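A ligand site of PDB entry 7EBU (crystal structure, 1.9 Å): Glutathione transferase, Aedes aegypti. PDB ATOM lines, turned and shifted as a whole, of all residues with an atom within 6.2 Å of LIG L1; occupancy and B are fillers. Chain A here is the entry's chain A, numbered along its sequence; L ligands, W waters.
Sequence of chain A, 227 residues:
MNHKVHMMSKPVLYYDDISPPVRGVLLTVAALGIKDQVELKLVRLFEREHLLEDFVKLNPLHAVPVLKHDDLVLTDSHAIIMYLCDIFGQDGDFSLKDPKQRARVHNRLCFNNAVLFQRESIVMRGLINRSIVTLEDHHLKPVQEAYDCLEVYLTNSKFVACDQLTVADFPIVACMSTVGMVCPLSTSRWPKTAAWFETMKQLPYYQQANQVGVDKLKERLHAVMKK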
ATOM      1  N   ILE A  18      25.903   2.983  -5.014  1.00  0.00           N
ATOM      2  CA  ILE A  18      26.066   3.551  -6.342  1.00  0.00           C
ATOM      3  C   ILE A  18      27.252   4.496  -6.423  1.00  0.00           C
ATOM      4  O   ILE A  18      27.801   4.715  -7.518  1.00  0.00           O
ATOM      5  CB  ILE A  18      24.734   4.204  -6.744  1.00  0.00           C
ATOM      6  CG1 ILE A  18      24.556   5.541  -6.011  1.00  0.00           C
ATOM      7  CG2 ILE A  18      23.577   3.247  -6.533  1.00  0.00           C
ATOM      8  CD1 ILE A  18      23.747   6.500  -6.786  1.00  0.00           C
ATOM      9  N   SER A  19      27.689   5.035  -5.302  1.00  0.00           N
ATOM     10  CA  SER A  19      28.805   5.963  -5.267  1.00  0.00           C
ATOM     11  C   SER A  19      30.127   5.212  -5.391  1.00  0.00           C
ATOM     12  O   SER A  19      30.371   4.275  -4.617  1.00  0.00           O
ATOM     13  CB  SER A  19      28.792   6.730  -3.956  1.00  0.00           C
ATOM     14  OG  SER A  19      30.077   7.231  -3.641  1.00  0.00           O
ATOM     15  N   PRO A  20      30.995   5.582  -6.334  1.00  0.00           N
ATOM     16  CA  PRO A  20      32.353   4.962  -6.422  1.00  0.00           C
ATOM     17  C   PRO A  20      33.142   5.099  -5.129  1.00  0.00           C
ATOM     18  O   PRO A  20      33.742   4.108  -4.677  1.00  0.00           O
ATOM     19  CB  PRO A  20      33.019   5.708  -7.577  1.00  0.00           C
ATOM     20  CG  PRO A  20      31.900   6.221  -8.409  1.00  0.00           C
ATOM     21  CD  PRO A  20      30.715   6.468  -7.473  1.00  0.00           C
ATOM     22  N   PRO A  21      33.229   6.285  -4.506  1.00  0.00           N
ATOM     23  CA  PRO A  21      33.929   6.351  -3.202  1.00  0.00           C
ATOM     24  C   PRO A  21      33.451   5.323  -2.183  1.00  0.00           C
ATOM     25  O   PRO A  21      34.247   4.682  -1.465  1.00  0.00           O
ATOM     26  CB  PRO A  21      33.638   7.776  -2.716  1.00  0.00           C
ATOM     27  CG  PRO A  21      33.524   8.558  -3.972  1.00  0.00           C
ATOM     28  CD  PRO A  21      32.824   7.638  -4.959  1.00  0.00           C
ATOM     29  N   ARG A  23      31.986   2.423  -2.871  1.00  0.00           N
ATOM     30  CA  ARG A  23      32.412   1.102  -3.299  1.00  0.00           C
ATOM     31  C   ARG A  23      33.898   0.875  -3.045  1.00  0.00           C
ATOM     32  O   ARG A  23      34.310  -0.253  -2.785  1.00  0.00           O
ATOM     33  CB  ARG A  23      32.035   0.908  -4.755  1.00  0.00           C
ATOM     34  CG  ARG A  23      30.539   0.642  -4.920  1.00  0.00           C
ATOM     35  CD  ARG A  23      30.171   0.301  -6.326  1.00  0.00           C
ATOM     36  NE  ARG A  23      29.742   1.482  -7.051  1.00  0.00           N
ATOM     37  CZ  ARG A  23      30.463   2.070  -7.998  1.00  0.00           C
ATOM     38  NH1 ARG A  23      31.658   1.605  -8.331  1.00  0.00           N
ATOM     39  NH2 ARG A  23      29.980   3.141  -8.603  1.00  0.00           N
ATOM     40  N   LEU A  45      21.139   8.314  -1.851  1.00  0.00           N
ATOM     41  CA  LEU A  45      21.333   9.610  -2.498  1.00  0.00           C
ATOM     42  C   LEU A  45      20.103  10.014  -3.309  1.00  0.00           C
ATOM     43  O   LEU A  45      19.642  11.156  -3.229  1.00  0.00           O
ATOM     44  CB  LEU A  45      22.578   9.558  -3.379  1.00  0.00           C
ATOM     45  CG  LEU A  45      23.902   9.370  -2.630  1.00  0.00           C
ATOM     46  CD1 LEU A  45      25.064   9.147  -3.613  1.00  0.00           C
ATOM     47  CD2 LEU A  45      24.183  10.546  -1.722  1.00  0.00           C
ATOM     48  N   PHE A  46      19.557   9.086  -4.101  1.00  0.00           N
ATOM     49  CA  PHE A  46      18.459   9.464  -4.982  1.00  0.00           C
ATOM     50  C   PHE A  46      17.181   9.776  -4.204  1.00  0.00           C
ATOM     51  O   PHE A  46      16.301  10.451  -4.723  1.00  0.00           O
ATOM     52  CB  PHE A  46      18.227   8.394  -6.039  1.00  0.00           C
ATOM     53  CG  PHE A  46      19.126   8.547  -7.252  1.00  0.00           C
ATOM     54  CD1 PHE A  46      18.900   9.551  -8.189  1.00  0.00           C
ATOM     55  CD2 PHE A  46      20.219   7.714  -7.424  1.00  0.00           C
ATOM     56  CE1 PHE A  46      19.737   9.692  -9.298  1.00  0.00           C
ATOM     57  CE2 PHE A  46      21.049   7.851  -8.521  1.00  0.00           C
ATOM     58  CZ  PHE A  46      20.811   8.837  -9.453  1.00  0.00           C
ATOM     59  N   GLU A  47      17.099   9.340  -2.949  1.00  0.00           N
ATOM     60  CA  GLU A  47      16.000   9.742  -2.083  1.00  0.00           C
ATOM     61  C   GLU A  47      16.303  11.009  -1.295  1.00  0.00           C
ATOM     62  O   GLU A  47      15.409  11.546  -0.625  1.00  0.00           O
ATOM     63  CB  GLU A  47      15.669   8.575  -1.143  1.00  0.00           C
ATOM     64  CG  GLU A  47      15.400   7.306  -1.948  1.00  0.00           C
ATOM     65  CD  GLU A  47      14.093   6.624  -1.582  1.00  0.00           C
ATOM     66  OE1 GLU A  47      13.963   6.265  -0.387  1.00  0.00           O
ATOM     67  OE2 GLU A  47      13.223   6.451  -2.468  1.00  0.00           O
ATOM     68  N   ARG A  48      17.549  11.504  -1.392  1.00  0.00           N
ATOM     69  CA  ARG A  48      18.048  12.706  -0.724  1.00  0.00           C
ATOM     70  C   ARG A  48      18.158  12.545   0.789  1.00  0.00           C
ATOM     71  O   ARG A  48      18.097  13.535   1.536  1.00  0.00           O
ATOM     72  CB  ARG A  48      17.220  13.942  -1.116  1.00  0.00           C
ATOM     73  CG  ARG A  48      17.432  14.273  -2.603  1.00  0.00           C
ATOM     74  CD  ARG A  48      16.664  15.514  -3.053  1.00  0.00           C
ATOM     75  NE  ARG A  48      15.286  15.464  -2.576  1.00  0.00           N
ATOM     76  CZ  ARG A  48      14.256  15.096  -3.319  1.00  0.00           C
ATOM     77  NH1 ARG A  48      14.390  14.769  -4.597  1.00  0.00           N
ATOM     78  NH2 ARG A  48      13.043  15.091  -2.776  1.00  0.00           N
ATOM     79  N   HIS A  50      20.821  12.070   2.237  1.00  0.00           N
ATOM     80  CA  HIS A  50      22.048  12.762   2.605  1.00  0.00           C
ATOM     81  C   HIS A  50      21.839  14.222   2.930  1.00  0.00           C
ATOM     82  O   HIS A  50      22.796  14.887   3.356  1.00  0.00           O
ATOM     83  CB  HIS A  50      23.096  12.634   1.470  1.00  0.00           C
ATOM     84  CG  HIS A  50      22.652  13.223   0.168  1.00  0.00           C
ATOM     85  ND1 HIS A  50      21.579  12.749  -0.550  1.00  0.00           N
ATOM     86  CD2 HIS A  50      23.171  14.241  -0.570  1.00  0.00           C
ATOM     87  CE1 HIS A  50      21.425  13.464  -1.648  1.00  0.00           C
ATOM     88  NE2 HIS A  50      22.393  14.370  -1.694  1.00  0.00           N
ATOM     89  N   LEU A  51      20.629  14.750   2.735  1.00  0.00           N
ATOM     90  CA  LEU A  51      20.337  16.144   3.042  1.00  0.00           C
ATOM     91  C   LEU A  51      19.525  16.295   4.327  1.00  0.00           C
ATOM     92  O   LEU A  51      19.157  17.408   4.669  1.00  0.00           O
ATOM     93  CB  LEU A  51      19.600  16.813   1.878  1.00  0.00           C
ATOM     94  CG  LEU A  51      20.325  16.737   0.517  1.00  0.00           C
ATOM     95  CD1 LEU A  51      19.477  17.296  -0.627  1.00  0.00           C
ATOM     96  CD2 LEU A  51      21.667  17.428   0.588  1.00  0.00           C
ATOM     97  N   PHE A 117      38.731  10.421  -9.655  1.00  0.00           N
ATOM     98  CA  PHE A 117      37.347  10.595  -9.236  1.00  0.00           C
ATOM     99  C   PHE A 117      36.824  11.997  -9.555  1.00  0.00           C
ATOM    100  O   PHE A 117      35.642  12.151  -9.871  1.00  0.00           O
ATOM    101  CB  PHE A 117      37.157  10.321  -7.744  1.00  0.00           C
ATOM    102  CG  PHE A 117      35.773  10.676  -7.250  1.00  0.00           C
ATOM    103  CD1 PHE A 117      34.679   9.917  -7.657  1.00  0.00           C
ATOM    104  CD2 PHE A 117      35.559  11.791  -6.448  1.00  0.00           C
ATOM    105  CE1 PHE A 117      33.396  10.238  -7.235  1.00  0.00           C
ATOM    106  CE2 PHE A 117      34.289  12.109  -6.027  1.00  0.00           C
ATOM    107  CZ  PHE A 117      33.214  11.331  -6.421  1.00  0.00           C
ATOM    108  N   GLU A 120      35.977  11.896 -13.281  1.00  0.00           N
ATOM    109  CA  GLU A 120      34.864  10.959 -13.394  1.00  0.00           C
ATOM    110  C   GLU A 120      33.561  11.601 -12.964  1.00  0.00           C
ATOM    111  O   GLU A 120      32.535  11.541 -13.674  1.00  0.00           O
ATOM    112  CB  GLU A 120      35.179   9.764 -12.503  1.00  0.00           C
ATOM    113  CG  GLU A 120      34.297   8.616 -12.653  1.00  0.00           C
ATOM    114  CD  GLU A 120      33.135   8.616 -11.716  1.00  0.00           C
ATOM    115  OE1 GLU A 120      33.189   9.179 -10.602  1.00  0.00           O
ATOM    116  OE2 GLU A 120      32.163   7.984 -12.090  1.00  0.00           O
ATOM    117  N   SER A 121      33.573  12.192 -11.772  1.00  0.00           N
ATOM    118  CA  SER A 121      32.406  12.766 -11.135  1.00  0.00           C
ATOM    119  C   SER A 121      31.820  13.876 -11.988  1.00  0.00           C
ATOM    120  O   SER A 121      30.604  13.977 -12.121  1.00  0.00           O
ATOM    121  CB  SER A 121      32.794  13.304  -9.764  1.00  0.00           C
ATOM    122  OG  SER A 121      31.653  13.732  -9.049  1.00  0.00           O
ATOM    123  N   ILE A 122      32.670  14.737 -12.538  1.00  0.00           N
ATOM    124  CA  ILE A 122      32.181  15.823 -13.386  1.00  0.00           C
ATOM    125  C   ILE A 122      31.240  15.265 -14.461  1.00  0.00           C
ATOM    126  O   ILE A 122      30.080  15.694 -14.592  1.00  0.00           O
ATOM    127  CB  ILE A 122      33.370  16.578 -14.006  1.00  0.00           C
ATOM    128  CG1 ILE A 122      33.817  17.682 -13.053  1.00  0.00           C
ATOM    129  CG2 ILE A 122      33.008  17.169 -15.363  1.00  0.00           C
ATOM    130  CD1 ILE A 122      35.294  18.005 -13.142  1.00  0.00           C
ATOM    131  N   MET A 124      29.815  12.152 -14.672  1.00  0.00           N
ATOM    132  CA  MET A 124      28.684  11.358 -14.209  1.00  0.00           C
ATOM    133  C   MET A 124      27.602  12.243 -13.593  1.00  0.00           C
ATOM    134  O   MET A 124      26.401  12.050 -13.870  1.00  0.00           O
ATOM    135  CB  MET A 124      29.122  10.285 -13.208  1.00  0.00           C
ATOM    136  CG  MET A 124      30.011   9.183 -13.792  1.00  0.00           C
ATOM    137  SD  MET A 124      29.444   8.451 -15.352  1.00  0.00           S
ATOM    138  CE  MET A 124      28.002   7.577 -14.770  1.00  0.00           C
ATOM    139  N   ARG A 125      27.980  13.200 -12.734  1.00  0.00           N
ATOM    140  CA  ARG A 125      26.995  14.163 -12.240  1.00  0.00           C
ATOM    141  C   ARG A 125      26.344  14.935 -13.382  1.00  0.00           C
ATOM    142  O   ARG A 125      25.135  15.189 -13.344  1.00  0.00           O
ATOM    143  CB  ARG A 125      27.592  15.160 -11.228  1.00  0.00           C
ATOM    144  CG  ARG A 125      27.996  14.587  -9.867  1.00  0.00           C
ATOM    145  CD  ARG A 125      28.827  15.551  -8.969  1.00  0.00           C
ATOM    146  NE  ARG A 125      29.253  16.782  -9.624  1.00  0.00           N
ATOM    147  CZ  ARG A 125      30.500  17.070  -9.964  1.00  0.00           C
ATOM    148  NH1 ARG A 125      31.525  16.376  -9.480  1.00  0.00           N
ATOM    149  NH2 ARG A 125      30.740  18.113 -10.760  1.00  0.00           N
ATOM    150  N   ILE A 128      23.756  12.571 -14.864  1.00  0.00           N
ATOM    151  CA  ILE A 128      22.731  12.281 -13.867  1.00  0.00           C
ATOM    152  C   ILE A 128      21.738  13.441 -13.745  1.00  0.00           C
ATOM    153  O   ILE A 128      20.530  13.230 -13.585  1.00  0.00           O
ATOM    154  CB  ILE A 128      23.385  11.968 -12.508  1.00  0.00           C
ATOM    155  CG1 ILE A 128      23.841  10.512 -12.448  1.00  0.00           C
ATOM    156  CG2 ILE A 128      22.438  12.264 -11.356  1.00  0.00           C
ATOM    157  CD1 ILE A 128      24.203  10.045 -11.034  1.00  0.00           C
ATOM    158  N   THR A 178      33.038   2.730 -13.102  1.00  0.00           N
ATOM    159  CA  THR A 178      31.898   3.630 -13.257  1.00  0.00           C
ATOM    160  C   THR A 178      32.032   4.402 -14.562  1.00  0.00           C
ATOM    161  O   THR A 178      31.180   4.280 -15.455  1.00  0.00           O
ATOM    162  CB  THR A 178      31.843   4.589 -12.069  1.00  0.00           C
ATOM    163  OG1 THR A 178      31.743   3.828 -10.860  1.00  0.00           O
ATOM    164  CG2 THR A 178      30.614   5.494 -12.180  1.00  0.00           C
ATOM    165  N   LEU A 217      23.774   1.916 -10.881  1.00  0.00           N
ATOM    166  CA  LEU A 217      24.054   3.180 -11.541  1.00  0.00           C
ATOM    167  C   LEU A 217      23.828   3.089 -13.040  1.00  0.00           C
ATOM    168  O   LEU A 217      23.355   4.052 -13.648  1.00  0.00           O
ATOM    169  CB  LEU A 217      25.481   3.634 -11.228  1.00  0.00           C
ATOM    170  CG  LEU A 217      25.838   4.998 -11.812  1.00  0.00           C
ATOM    171  CD1 LEU A 217      24.926   6.073 -11.241  1.00  0.00           C
ATOM    172  CD2 LEU A 217      27.286   5.345 -11.539  1.00  0.00           C
HETATM  173  O1  LIG L   1      30.137   8.262 -10.110  1.00  0.00           O
HETATM  174  C1  LIG L   1      29.181   9.050  -9.589  1.00  0.00           C
HETATM  175  C2  LIG L   1      29.371  10.443  -9.574  1.00  0.00           C
HETATM  176  C3  LIG L   1      28.392  11.281  -9.033  1.00  0.00           C
HETATM  177  C4  LIG L   1      27.229  10.721  -8.513  1.00  0.00           C
HETATM  178  C5  LIG L   1      27.040   9.238  -8.522  1.00  0.00           C
HETATM  179  C6  LIG L   1      28.035   8.443  -9.066  1.00  0.00           C
HETATM  180  O2  LIG L   1      25.895   8.698  -8.002  1.00  0.00           O
HETATM  181  C7  LIG L   1      24.915   9.439  -7.467  1.00  0.00           C
HETATM  182  C8  LIG L   1      24.967  10.826  -7.381  1.00  0.00           C
HETATM  183  C9  LIG L   1      26.156  11.528  -7.908  1.00  0.00           C
HETATM  184  O3  LIG L   1      26.254  12.764  -7.870  1.00  0.00           O
HETATM  185  C10 LIG L   1      23.811  11.557  -6.772  1.00  0.00           C
HETATM  186  C11 LIG L   1      22.517  11.202  -7.138  1.00  0.00           C
HETATM  187  C12 LIG L   1      21.426  11.873  -6.595  1.00  0.00           C
HETATM  188  C13 LIG L   1      21.622  12.895  -5.675  1.00  0.00           C
HETATM  189  O4  LIG L   1      20.553  13.546  -5.161  1.00  0.00           O
HETATM  190  C14 LIG L   1      22.922  13.273  -5.308  1.00  0.00           C
HETATM  191  C15 LIG L   1      24.016  12.589  -5.852  1.00  0.00           C
HETATM  192  N1  LG2 L   2      36.188  12.835  -1.918  1.00  0.00           N
HETATM  193  C1  LG2 L   2      34.945  12.184  -1.397  1.00  0.00           C
HETATM  194  C2  LG2 L   2      35.206  10.734  -0.971  1.00  0.00           C
HETATM  195  O1  LG2 L   2      36.090  10.098  -1.595  1.00  0.00           O
HETATM  196  O2  LG2 L   2      34.513  10.266  -0.029  1.00  0.00           O
HETATM  197  C3  LG2 L   2      33.841  12.290  -2.452  1.00  0.00           C
HETATM  198  C4  LG2 L   2      32.507  11.718  -1.982  1.00  0.00           C
HETATM  199  C5  LG2 L   2      31.385  12.091  -2.919  1.00  0.00           C
HETATM  200  O3  LG2 L   2      31.508  12.954  -3.779  1.00  0.00           O
HETATM  201  N2  LG2 L   2      30.243  11.415  -2.762  1.00  0.00           N
HETATM  202  C6  LG2 L   2      29.079  11.639  -3.586  1.00  0.00           C
HETATM  203  C7  LG2 L   2      27.882  12.207  -2.824  1.00  0.00           C
HETATM  204  O4  LG2 L   2      27.556  11.678  -1.761  1.00  0.00           O
HETATM  205  C8  LG2 L   2      28.640  10.382  -4.313  1.00  0.00           C
HETATM  206  S1  LG2 L   2      29.841   9.797  -5.534  1.00  0.00           S
HETATM  207  N3  LG2 L   2      27.235  13.219  -3.397  1.00  0.00           N
HETATM  208  C9  LG2 L   2      26.067  13.843  -2.795  1.00  0.00           C
HETATM  209  C10 LG2 L   2      26.194  15.366  -2.775  1.00  0.00           C
HETATM  210  O5  LG2 L   2      27.205  15.847  -3.313  1.00  0.00           O
HETATM  211  O6  LG2 L   2      25.266  16.018  -2.239  1.00  0.00           O
HETATM  212  O   HOH W   1      17.923  12.908  -6.188  1.00  0.00           O
HETATM  213  O   HOH W   2      21.824  16.221  -3.963  1.00  0.00           O
HETATM  214  O   HOH W   3      27.743  13.945  -6.048  1.00  0.00           O
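Water W3 bridges an oxygen (O3) of LIG L1 and a nitrogen (N3) of LG2 L2. Water W1 lies within hydrogen-bond range of an oxygen (O4) of LIG L1 (2.9 Å) and the backbone carbonyl oxygen (O) of Phe 46 (3.3 Å). Water W2 bridges NE2 of His 50 (3.0 Å) and O4 of LIG L1 (3.2 Å).
Merely in contact with LIG L1: Pro 20 (3.2 Å), Arg 125 (3.2 Å), Ile 18 (3.2 Å), Thr 178 (3.5 Å), His 50 (3.6 Å), Met 124 (3.6 Å), Ile 128 (3.7 Å) and Phe 46 (3.7 Å). Hydrophobic or aromatic side chains within 4 Å of LIG L1: Ile 18, Pro 20, Leu 45, Phe 46, His 50, Met 124 and Ile 128. Of the 20 residues printed, 10 come within 4 Å of LIG L1.
OE2 of Glu 120 sits at hydrogen-bond distance from O1 of LIG L1, 2.8 Å away. O of Leu 45 is in hydrogen-bond range of O4 of LIG L1 (3.2 Å). A ring nitrogen (NE2) of His 50 lies close to an oxygen (O6) of LG2 L2, 3.4 Å away. A sulfur (S1) of LG2 L2 sits close to the side-chain hydroxyl (OG) of Ser 19, at 3.2 Å.
NH1 of Arg 125 lies within hydrogen-bond range of OG of Ser 121, at 2.7 Å. The backbone carbonyl oxygen of Ile 18 lies within hydrogen-bond range of the guanidinium group of Arg 23 (2.9 Å). The side-chain hydroxyl (OG1) of Thr 178 is in hydrogen-bond range of the guanidinium group (NH2) of Arg 23, 2.9 Å away.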
